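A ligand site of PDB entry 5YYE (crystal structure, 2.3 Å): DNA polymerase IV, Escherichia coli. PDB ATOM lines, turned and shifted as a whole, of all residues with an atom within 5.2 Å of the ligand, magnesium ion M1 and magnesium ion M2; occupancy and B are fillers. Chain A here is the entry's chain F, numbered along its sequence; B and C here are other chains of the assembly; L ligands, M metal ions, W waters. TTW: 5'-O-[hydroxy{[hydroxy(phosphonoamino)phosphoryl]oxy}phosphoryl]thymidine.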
ATOM      1  N   ASP A   9      22.676 -21.965 -24.677  1.00  0.00           N
ATOM      2  CA  ASP A   9      21.464 -22.741 -24.431  1.00  0.00           C
ATOM      3  C   ASP A   9      21.820 -24.217 -24.531  1.00  0.00           C
ATOM      4  O   ASP A   9      22.283 -24.662 -25.591  1.00  0.00           O
ATOM      5  CB  ASP A   9      20.365 -22.353 -25.414  1.00  0.00           C
ATOM      6  CG  ASP A   9      18.983 -22.876 -25.010  1.00  0.00           C
ATOM      7  OD1 ASP A   9      18.875 -24.086 -24.725  1.00  0.00           O
ATOM      8  OD2 ASP A   9      18.019 -22.092 -24.995  1.00  0.00           O
ATOM      9  N   MET A  10      21.590 -24.967 -23.445  1.00  0.00           N
ATOM     10  CA  MET A  10      21.857 -26.406 -23.436  1.00  0.00           C
ATOM     11  C   MET A  10      20.929 -27.137 -24.410  1.00  0.00           C
ATOM     12  O   MET A  10      19.766 -26.767 -24.586  1.00  0.00           O
ATOM     13  CB  MET A  10      21.682 -26.987 -22.030  1.00  0.00           C
ATOM     14  CG  MET A  10      22.636 -26.393 -20.997  1.00  0.00           C
ATOM     15  SD  MET A  10      24.361 -26.433 -21.457  1.00  0.00           S
ATOM     16  CE  MET A  10      24.733 -28.151 -21.234  1.00  0.00           C
ATOM     17  N   ASP A  11      21.457 -28.196 -25.046  1.00  0.00           N
ATOM     18  CA  ASP A  11      20.686 -28.980 -26.005  1.00  0.00           C
ATOM     19  C   ASP A  11      19.863 -30.041 -25.269  1.00  0.00           C
ATOM     20  O   ASP A  11      20.410 -30.815 -24.478  1.00  0.00           O
ATOM     21  CB  ASP A  11      21.595 -29.653 -27.038  1.00  0.00           C
ATOM     22  CG  ASP A  11      22.487 -28.647 -27.803  1.00  0.00           C
ATOM     23  OD1 ASP A  11      21.959 -27.640 -28.335  1.00  0.00           O
ATOM     24  OD2 ASP A  11      23.714 -28.854 -27.845  1.00  0.00           O
ATOM     25  N   CYS A  12      18.555 -30.045 -25.516  1.00  0.00           N
ATOM     26  CA  CYS A  12      17.617 -30.979 -24.887  1.00  0.00           C
ATOM     27  C   CYS A  12      17.983 -31.266 -23.418  1.00  0.00           C
ATOM     28  O   CYS A  12      18.110 -32.427 -23.004  1.00  0.00           O
ATOM     29  CB  CYS A  12      17.543 -32.277 -25.698  1.00  0.00           C
ATOM     30  SG  CYS A  12      17.058 -31.961 -27.380  1.00  0.00           S
ATOM     31  N   PHE A  13      18.124 -30.176 -22.649  1.00  0.00           N
ATOM     32  CA  PHE A  13      18.885 -30.184 -21.401  1.00  0.00           C
ATOM     33  C   PHE A  13      18.564 -31.388 -20.510  1.00  0.00           C
ATOM     34  O   PHE A  13      19.463 -32.187 -20.181  1.00  0.00           O
ATOM     35  CB  PHE A  13      18.671 -28.876 -20.651  1.00  0.00           C
ATOM     36  CG  PHE A  13      19.439 -28.799 -19.367  1.00  0.00           C
ATOM     37  CD1 PHE A  13      20.756 -29.256 -19.297  1.00  0.00           C
ATOM     38  CD2 PHE A  13      18.855 -28.283 -18.219  1.00  0.00           C
ATOM     39  CE1 PHE A  13      21.466 -29.197 -18.109  1.00  0.00           C
ATOM     40  CE2 PHE A  13      19.576 -28.206 -17.024  1.00  0.00           C
ATOM     41  CZ  PHE A  13      20.863 -28.667 -16.960  1.00  0.00           C
ATOM     42  N   PHE A  14      17.301 -31.545 -20.087  1.00  0.00           N
ATOM     43  CA  PHE A  14      16.969 -32.677 -19.206  1.00  0.00           C
ATOM     44  C   PHE A  14      17.276 -34.005 -19.884  1.00  0.00           C
ATOM     45  O   PHE A  14      17.881 -34.900 -19.284  1.00  0.00           O
ATOM     46  CB  PHE A  14      15.503 -32.663 -18.775  1.00  0.00           C
ATOM     47  CG  PHE A  14      15.106 -31.532 -17.877  1.00  0.00           C
ATOM     48  CD1 PHE A  14      15.942 -30.450 -17.660  1.00  0.00           C
ATOM     49  CD2 PHE A  14      13.869 -31.535 -17.260  1.00  0.00           C
ATOM     50  CE1 PHE A  14      15.536 -29.403 -16.833  1.00  0.00           C
ATOM     51  CE2 PHE A  14      13.468 -30.501 -16.433  1.00  0.00           C
ATOM     52  CZ  PHE A  14      14.294 -29.438 -16.222  1.00  0.00           C
ATOM     53  N   ALA A  15      16.821 -34.158 -21.127  1.00  0.00           N
ATOM     54  CA  ALA A  15      17.096 -35.397 -21.849  1.00  0.00           C
ATOM     55  C   ALA A  15      18.598 -35.652 -21.980  1.00  0.00           C
ATOM     56  O   ALA A  15      19.083 -36.764 -21.720  1.00  0.00           O
ATOM     57  CB  ALA A  15      16.418 -35.375 -23.222  1.00  0.00           C
ATOM     58  N   ILE A  42       5.023 -33.389 -21.646  1.00  0.00           N
ATOM     59  CA  ILE A  42       6.440 -33.551 -21.898  1.00  0.00           C
ATOM     60  C   ILE A  42       7.162 -32.321 -21.378  1.00  0.00           C
ATOM     61  O   ILE A  42       6.798 -31.188 -21.730  1.00  0.00           O
ATOM     62  CB  ILE A  42       6.687 -33.759 -23.394  1.00  0.00           C
ATOM     63  CG1 ILE A  42       5.916 -34.996 -23.860  1.00  0.00           C
ATOM     64  CG2 ILE A  42       8.185 -33.879 -23.707  1.00  0.00           C
ATOM     65  CD1 ILE A  42       6.244 -36.237 -23.046  1.00  0.00           C
ATOM     66  N   SER A  43       8.147 -32.521 -20.520  1.00  0.00           N
ATOM     67  CA  SER A  43       9.069 -31.425 -20.208  1.00  0.00           C
ATOM     68  C   SER A  43       9.982 -31.200 -21.401  1.00  0.00           C
ATOM     69  O   SER A  43       9.957 -30.142 -22.041  1.00  0.00           O
ATOM     70  CB  SER A  43       9.864 -31.739 -18.945  1.00  0.00           C
ATOM     71  OG  SER A  43       9.334 -31.041 -17.836  1.00  0.00           O
ATOM     72  N   THR A  44      10.791 -32.199 -21.731  1.00  0.00           N
ATOM     73  CA  THR A  44      11.582 -32.166 -22.939  1.00  0.00           C
ATOM     74  C   THR A  44      11.770 -33.595 -23.418  1.00  0.00           C
ATOM     75  O   THR A  44      11.332 -34.547 -22.754  1.00  0.00           O
ATOM     76  CB  THR A  44      12.918 -31.481 -22.719  1.00  0.00           C
ATOM     77  OG1 THR A  44      13.475 -31.165 -23.998  1.00  0.00           O
ATOM     78  CG2 THR A  44      13.888 -32.375 -21.973  1.00  0.00           C
ATOM     79  N   TYR A  47      16.354 -36.180 -29.457  1.00  0.00           N
ATOM     80  CA  TYR A  47      16.087 -36.016 -30.887  1.00  0.00           C
ATOM     81  C   TYR A  47      15.442 -37.264 -31.520  1.00  0.00           C
ATOM     82  O   TYR A  47      14.516 -37.119 -32.319  1.00  0.00           O
ATOM     83  CB  TYR A  47      17.375 -35.594 -31.589  1.00  0.00           C
ATOM     84  CG  TYR A  47      17.616 -34.079 -31.538  1.00  0.00           C
ATOM     85  CD1 TYR A  47      16.795 -33.211 -32.234  1.00  0.00           C
ATOM     86  CD2 TYR A  47      18.655 -33.539 -30.793  1.00  0.00           C
ATOM     87  CE1 TYR A  47      16.993 -31.834 -32.190  1.00  0.00           C
ATOM     88  CE2 TYR A  47      18.862 -32.159 -30.738  1.00  0.00           C
ATOM     89  CZ  TYR A  47      18.028 -31.326 -31.451  1.00  0.00           C
ATOM     90  OH  TYR A  47      18.202 -29.965 -31.429  1.00  0.00           O
ATOM     91  N   ARG A  50      11.748 -36.374 -30.871  1.00  0.00           N
ATOM     92  CA  ARG A  50      11.182 -35.323 -31.725  1.00  0.00           C
ATOM     93  C   ARG A  50      11.184 -35.689 -33.218  1.00  0.00           C
ATOM     94  O   ARG A  50      10.453 -35.057 -33.992  1.00  0.00           O
ATOM     95  CB  ARG A  50      11.905 -33.997 -31.503  1.00  0.00           C
ATOM     96  CG  ARG A  50      13.249 -34.107 -30.890  1.00  0.00           C
ATOM     97  CD  ARG A  50      13.778 -32.743 -30.486  1.00  0.00           C
ATOM     98  NE  ARG A  50      13.237 -32.323 -29.203  1.00  0.00           N
ATOM     99  CZ  ARG A  50      13.669 -31.275 -28.518  1.00  0.00           C
ATOM    100  NH1 ARG A  50      14.651 -30.526 -29.009  1.00  0.00           N
ATOM    101  NH2 ARG A  50      13.124 -30.980 -27.371  1.00  0.00           N
ATOM    102  N   SER A  56       8.102 -30.222 -26.399  1.00  0.00           N
ATOM    103  CA  SER A  56       7.826 -29.669 -25.074  1.00  0.00           C
ATOM    104  C   SER A  56       6.399 -29.140 -24.992  1.00  0.00           C
ATOM    105  O   SER A  56       5.878 -28.569 -25.956  1.00  0.00           O
ATOM    106  CB  SER A  56       8.811 -28.531 -24.781  1.00  0.00           C
ATOM    107  OG  SER A  56       9.971 -29.019 -24.157  1.00  0.00           O
ATOM    108  N   ALA A  57       5.780 -29.300 -23.823  1.00  0.00           N
ATOM    109  CA  ALA A  57       4.426 -28.835 -23.503  1.00  0.00           C
ATOM    110  C   ALA A  57       3.335 -29.641 -24.216  1.00  0.00           C
ATOM    111  O   ALA A  57       2.172 -29.249 -24.167  1.00  0.00           O
ATOM    112  CB  ALA A  57       4.238 -27.345 -23.820  1.00  0.00           C
ATOM    113  N   SER A 102      16.929 -19.522 -16.814  1.00  0.00           N
ATOM    114  CA  SER A 102      16.378 -20.813 -16.413  1.00  0.00           C
ATOM    115  C   SER A 102      17.578 -21.633 -16.011  1.00  0.00           C
ATOM    116  O   SER A 102      18.711 -21.133 -16.017  1.00  0.00           O
ATOM    117  CB  SER A 102      15.562 -21.454 -17.552  1.00  0.00           C
ATOM    118  OG  SER A 102      16.395 -21.689 -18.699  1.00  0.00           O
ATOM    119  N   ASP A 104      19.044 -23.805 -17.824  1.00  0.00           N
ATOM    120  CA  ASP A 104      19.851 -24.272 -18.940  1.00  0.00           C
ATOM    121  C   ASP A 104      20.341 -23.167 -19.875  1.00  0.00           C
ATOM    122  O   ASP A 104      20.944 -23.489 -20.915  1.00  0.00           O
ATOM    123  CB  ASP A 104      19.083 -25.335 -19.726  1.00  0.00           C
ATOM    124  CG  ASP A 104      18.406 -24.806 -20.985  1.00  0.00           C
ATOM    125  OD1 ASP A 104      17.871 -23.678 -20.999  1.00  0.00           O
ATOM    126  OD2 ASP A 104      18.405 -25.543 -21.995  1.00  0.00           O
ATOM    127  N   GLU A 105      20.137 -21.899 -19.549  1.00  0.00           N
ATOM    128  CA  GLU A 105      20.499 -20.837 -20.479  1.00  0.00           C
ATOM    129  C   GLU A 105      20.869 -19.557 -19.716  1.00  0.00           C
ATOM    130  O   GLU A 105      20.570 -19.403 -18.526  1.00  0.00           O
ATOM    131  CB  GLU A 105      19.388 -20.610 -21.510  1.00  0.00           C
ATOM    132  CG  GLU A 105      18.110 -20.032 -21.006  1.00  0.00           C
ATOM    133  CD  GLU A 105      17.100 -19.861 -22.125  1.00  0.00           C
ATOM    134  OE1 GLU A 105      16.740 -20.875 -22.772  1.00  0.00           O
ATOM    135  OE2 GLU A 105      16.647 -18.728 -22.386  1.00  0.00           O
ATOM    136  N   ASP A 155      19.068 -20.752 -31.517  1.00  0.00           N
ATOM    137  CA  ASP A 155      18.325 -21.884 -32.011  1.00  0.00           C
ATOM    138  C   ASP A 155      18.659 -22.251 -33.450  1.00  0.00           C
ATOM    139  O   ASP A 155      18.351 -23.367 -33.888  1.00  0.00           O
ATOM    140  CB  ASP A 155      16.814 -21.641 -31.897  1.00  0.00           C
ATOM    141  CG  ASP A 155      16.312 -21.629 -30.463  1.00  0.00           C
ATOM    142  OD1 ASP A 155      17.030 -22.112 -29.547  1.00  0.00           O
ATOM    143  OD2 ASP A 155      15.195 -21.127 -30.251  1.00  0.00           O
ATOM    144  N   LYS A 158      21.226 -25.165 -33.601  1.00  0.00           N
ATOM    145  CA  LYS A 158      21.054 -26.142 -32.545  1.00  0.00           C
ATOM    146  C   LYS A 158      20.853 -27.518 -33.219  1.00  0.00           C
ATOM    147  O   LYS A 158      20.240 -27.588 -34.279  1.00  0.00           O
ATOM    148  CB  LYS A 158      19.864 -25.710 -31.678  1.00  0.00           C
ATOM    149  CG  LYS A 158      19.725 -26.410 -30.357  1.00  0.00           C
ATOM    150  CD  LYS A 158      18.682 -25.715 -29.474  1.00  0.00           C
ATOM    151  CE  LYS A 158      19.330 -24.762 -28.477  1.00  0.00           C
ATOM    152  NZ  LYS A 158      19.957 -25.496 -27.319  1.00  0.00           N
ATOM    153  P    DC B  18      11.926 -19.843 -23.954  1.00  0.00           P
ATOM    154  OP1  DC B  18      13.235 -19.637 -24.592  1.00  0.00           O
ATOM    155  OP2  DC B  18      10.869 -20.550 -24.707  1.00  0.00           O
ATOM    156  O5'  DC B  18      12.208 -20.653 -22.608  1.00  0.00           O
ATOM    157  C5'  DC B  18      13.263 -20.240 -21.745  1.00  0.00           C
ATOM    158  C4'  DC B  18      13.376 -21.208 -20.586  1.00  0.00           C
ATOM    159  O4'  DC B  18      12.144 -21.176 -19.830  1.00  0.00           O
ATOM    160  C3'  DC B  18      13.585 -22.652 -21.014  1.00  0.00           C
ATOM    161  O3'  DC B  18      14.937 -22.957 -20.972  1.00  0.00           O
ATOM    162  C2'  DC B  18      12.832 -23.456 -19.928  1.00  0.00           C
ATOM    163  C1'  DC B  18      11.816 -22.471 -19.375  1.00  0.00           C
ATOM    164  N1   DC B  18      10.416 -22.774 -19.723  1.00  0.00           N
ATOM    165  C2   DC B  18       9.688 -23.619 -18.876  1.00  0.00           C
ATOM    166  O2   DC B  18      10.270 -24.121 -17.902  1.00  0.00           O
ATOM    167  N3   DC B  18       8.389 -23.893 -19.153  1.00  0.00           N
ATOM    168  C4   DC B  18       7.804 -23.344 -20.207  1.00  0.00           C
ATOM    169  N4   DC B  18       6.503 -23.651 -20.420  1.00  0.00           N
ATOM    170  C5   DC B  18       8.524 -22.484 -21.122  1.00  0.00           C
ATOM    171  C6   DC B  18       9.811 -22.201 -20.822  1.00  0.00           C
ATOM    172  P    DA C   4      -1.693 -29.658 -17.763  1.00  0.00           P
ATOM    173  OP1  DA C   4      -2.731 -30.230 -16.902  1.00  0.00           O
ATOM    174  OP2  DA C   4      -1.753 -28.188 -18.035  1.00  0.00           O
ATOM    175  O5'  DA C   4      -0.292 -30.057 -17.165  1.00  0.00           O
ATOM    176  C5'  DA C   4      -0.035 -31.384 -16.829  1.00  0.00           C
ATOM    177  C4'  DA C   4       1.063 -31.464 -15.771  1.00  0.00           C
ATOM    178  O4'  DA C   4       2.351 -31.077 -16.358  1.00  0.00           O
ATOM    179  C3'  DA C   4       0.870 -30.553 -14.575  1.00  0.00           C
ATOM    180  O3'  DA C   4       1.424 -31.148 -13.433  1.00  0.00           O
ATOM    181  C2'  DA C   4       1.641 -29.275 -14.963  1.00  0.00           C
ATOM    182  C1'  DA C   4       2.771 -29.814 -15.841  1.00  0.00           C
ATOM    183  N9   DA C   4       3.073 -28.951 -16.964  1.00  0.00           N
ATOM    184  C8   DA C   4       2.189 -28.205 -17.699  1.00  0.00           C
ATOM    185  N7   DA C   4       2.749 -27.535 -18.675  1.00  0.00           N
ATOM    186  C5   DA C   4       4.077 -27.875 -18.581  1.00  0.00           C
ATOM    187  C6   DA C   4       5.209 -27.520 -19.342  1.00  0.00           C
ATOM    188  N6   DA C   4       5.170 -26.673 -20.391  1.00  0.00           N
ATOM    189  N1   DA C   4       6.382 -28.038 -18.967  1.00  0.00           N
ATOM    190  C2   DA C   4       6.430 -28.874 -17.935  1.00  0.00           C
ATOM    191  N3   DA C   4       5.430 -29.307 -17.153  1.00  0.00           N
ATOM    192  C4   DA C   4       4.284 -28.755 -17.529  1.00  0.00           C
ATOM    193  P    DG C   5       1.296 -30.395 -12.024  1.00  0.00           P
ATOM    194  OP1  DG C   5       1.370 -31.404 -10.951  1.00  0.00           O
ATOM    195  OP2  DG C   5       0.121 -29.492 -12.153  1.00  0.00           O
ATOM    196  O5'  DG C   5       2.617 -29.528 -11.926  1.00  0.00           O
ATOM    197  C5'  DG C   5       3.834 -30.155 -11.619  1.00  0.00           C
ATOM    198  C4'  DG C   5       4.932 -29.139 -11.566  1.00  0.00           C
ATOM    199  O4'  DG C   5       5.123 -28.532 -12.874  1.00  0.00           O
ATOM    200  C3'  DG C   5       4.662 -27.990 -10.604  1.00  0.00           C
ATOM    201  O3'  DG C   5       5.837 -27.730  -9.888  1.00  0.00           O
ATOM    202  C2'  DG C   5       4.289 -26.823 -11.527  1.00  0.00           C
ATOM    203  C1'  DG C   5       5.151 -27.127 -12.740  1.00  0.00           C
ATOM    204  N9   DG C   5       4.692 -26.491 -13.977  1.00  0.00           N
ATOM    205  C8   DG C   5       3.396 -26.218 -14.381  1.00  0.00           C
ATOM    206  N7   DG C   5       3.314 -25.656 -15.562  1.00  0.00           N
ATOM    207  C5   DG C   5       4.667 -25.525 -15.956  1.00  0.00           C
ATOM    208  C6   DG C   5       5.238 -24.956 -17.137  1.00  0.00           C
ATOM    209  O6   DG C   5       4.651 -24.442 -18.111  1.00  0.00           O
ATOM    210  N1   DG C   5       6.623 -25.035 -17.120  1.00  0.00           N
ATOM    211  C2   DG C   5       7.376 -25.591 -16.114  1.00  0.00           C
ATOM    212  N2   DG C   5       8.723 -25.579 -16.279  1.00  0.00           N
ATOM    213  N3   DG C   5       6.845 -26.111 -15.009  1.00  0.00           N
ATOM    214  C4   DG C   5       5.502 -26.047 -14.999  1.00  0.00           C
HETATM  215  O4  TTW L   1       8.014 -26.131 -21.676  1.00  0.00           O
HETATM  216  C4  TTW L   1       9.003 -26.493 -21.144  1.00  0.00           C
HETATM  217  N3  TTW L   1       8.982 -27.274 -20.068  1.00  0.00           N
HETATM  218  C2  TTW L   1      10.113 -27.648 -19.503  1.00  0.00           C
HETATM  219  O2  TTW L   1      10.061 -28.361 -18.562  1.00  0.00           O
HETATM  220  C5  TTW L   1      10.209 -26.103 -21.665  1.00  0.00           C
HETATM  221  C5M TTW L   1      10.230 -25.208 -22.929  1.00  0.00           C
HETATM  222  C6  TTW L   1      11.385 -26.522 -21.068  1.00  0.00           C
HETATM  223  N1  TTW L   1      11.289 -27.288 -19.976  1.00  0.00           N
HETATM  224  C1' TTW L   1      12.512 -27.789 -19.349  1.00  0.00           C
HETATM  225  O4' TTW L   1      13.695 -26.753 -19.513  1.00  0.00           O
HETATM  226  C2' TTW L   1      12.916 -28.904 -19.998  1.00  0.00           C
HETATM  227  C3' TTW L   1      14.081 -28.523 -20.904  1.00  0.00           C
HETATM  228  O3' TTW L   1      15.063 -29.476 -21.067  1.00  0.00           O
HETATM  229  C4' TTW L   1      14.690 -27.317 -20.137  1.00  0.00           C
HETATM  230  C5' TTW L   1      15.354 -26.323 -21.151  1.00  0.00           C
HETATM  231  O5' TTW L   1      14.347 -25.725 -21.896  1.00  0.00           O
HETATM  232  PA  TTW L   1      14.652 -25.412 -23.498  1.00  0.00           P
HETATM  233  O1A TTW L   1      13.622 -24.449 -24.067  1.00  0.00           O
HETATM  234  O2A TTW L   1      16.098 -24.837 -23.615  1.00  0.00           O
HETATM  235  O3A TTW L   1      14.568 -26.785 -24.426  1.00  0.00           O
HETATM  236  PB  TTW L   1      15.571 -28.103 -24.356  1.00  0.00           P
HETATM  237  O1B TTW L   1      15.043 -29.307 -23.618  1.00  0.00           O
HETATM  238  O2B TTW L   1      16.854 -27.739 -23.672  1.00  0.00           O
HETATM  239  N3B TTW L   1      15.780 -28.418 -26.037  1.00  0.00           N
HETATM  240  PG  TTW L   1      16.621 -27.275 -26.940  1.00  0.00           P
HETATM  241  O1G TTW L   1      17.785 -28.035 -27.478  1.00  0.00           O
HETATM  242  O2G TTW L   1      17.088 -26.073 -26.149  1.00  0.00           O
HETATM  243  O3G TTW L   1      15.658 -26.770 -27.961  1.00  0.00           O
HETATM  244 MG    MG M   1      17.847 -25.932 -24.048  1.00  0.00          MG
HETATM  245 MG    MG M   2      16.575 -22.772 -22.598  1.00  0.00          MG
HETATM  246  O   HOH W   1      15.977 -23.894 -26.930  1.00  0.00           O
HETATM  247  O   HOH W   2      15.193 -22.104 -24.804  1.00  0.00           O
HETATM  248  O   HOH W   3       6.905 -24.745 -23.543  1.00  0.00           O
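Magnesium ion M1 is bound by an oxygen (O2B) of the ligand (2.1 Å), an oxygen (O2A) of the ligand (2.1 Å), the backbone carbonyl oxygen (O) of Met 10 (2.2 Å), the side-chain carboxylate (OD2) of Asp 104 (2.2 Å), the side-chain carboxylate (OD1) of Asp 9 (2.2 Å) and an oxygen (O2G) of the ligand (2.2 Å).
Magnesium ion M1 has six donor atoms within binding distance.
OG1 of Thr 44 is in hydrogen-bond range of O1B of the ligand, 2.5 Å away.
The side-chain hydroxyl (OG) of Ser 43 sits at hydrogen-bond distance from an oxygen (O2) of the ligand (2.9 Å).
The backbone NH of Cys 12 lies within hydrogen-bond range of an oxygen (O1G) of the ligand (2.9 Å).
N1 of DA 4 of chain C sits at hydrogen-bond distance from N3 of the ligand, 2.9 Å away.
The backbone NH of Phe 13 is in hydrogen-bond range of an oxygen (O1B) of the ligand (3.3 Å).
The side-chain amino group (NZ) of Lys 158 lies within salt-bridge range of an oxygen (O1G) of the ligand (3.3 Å).
O3' of the ligand lies within hydrogen-bond range of N of Phe 14 (3.2 Å).
The backbone carbonyl oxygen of Met 10 lies close to the side-chain amino group of Lys 158, 3.0 Å away.
The side-chain carboxylate (OD1) of Asp 104 lies close to the side-chain hydroxyl (OG) of Ser 102 (3.4 Å).
The backbone carbonyl oxygen (O) of Asp 9 is in hydrogen-bond range of the side-chain amino group (NZ) of Lys 158 (3.0 Å).
O2 of DC 18 of chain B sits close to N2 of DG 5 of chain C (2.7 Å).
O3' of DC 18 of chain B sits close to the side-chain hydroxyl (OG) of Ser 102 (3.0 Å).
The guanidinium group of Arg 50 is in hydrogen-bond range of the side-chain hydroxyl of Thr 44, 3.4 Å away.
SG of Cys 12 is in hydrogen-bond range of NH1 of Arg 50.
The side-chain carboxylate (OD1) of Asp 11 lies within salt-bridge range of the side-chain amino group (NZ) of Lys 158, 3.1 Å away.
OE1 of Glu 105 is bound to magnesium ion M2, 1.9 Å away.
OD1 of Asp 104 is bound to magnesium ion M2 (2.2 Å).
O3' of DC 18 of chain B binds magnesium ion M2 (2.3 Å).
Magnesium ion M2 is bound by an oxygen (O2A) of the ligand, 2.4 Å away.
Slightly farther from magnesium ion M2 lies water W2 (2.7 Å).
Of the 22 residues printed, 4 come within 4 Å of magnesium ion M2.
The nearest printed residue that does not touch magnesium ion M2 is Ser 102 (4.1 Å).
Water W2 lies within hydrogen-bond range of OD2 of Asp 9 (2.8 Å), O1A of the ligand (2.9 Å) and OP1 of DC 18 of chain B (3.2 Å).
Water W1 lies within hydrogen-bond range of an oxygen (O3G) of the ligand (3.1 Å), the side-chain carboxylate of Asp 155 (3.3 Å) and the side-chain carboxylate of Asp 9 (3.3 Å).
Water W3 lies within hydrogen-bond range of an oxygen (O4) of the ligand (2.6 Å) and N4 of DC 18 of chain B (3.3 Å).
Lys 158 touches magnesium ion M1 (NZ to MG, 3.9 Å).
Of the 22 residues printed, 4 come within 4 Å of magnesium ion M1.
Merely in contact with the ligand: Asp 11 (3.4 Å), Arg 50 (3.8 Å), Ser 56 (3.8 Å) and DG 5 of chain C (3.8 Å).
Hydrophobic or aromatic side chains that line the ligand: Phe 13 and Phe 14.
Within 4 Å of the ligand: Asp 9, Met 10, Asp 11, Cys 12, Phe 13, Phe 14, Ser 43, Thr 44, Arg 50, Ser 56, Asp 104, Lys 158, DC 18 of chain B, DA 4 of chain C and DG 5 of chain C.
The nearest printed residue that does not touch the ligand is Glu 105 (4.1 Å).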
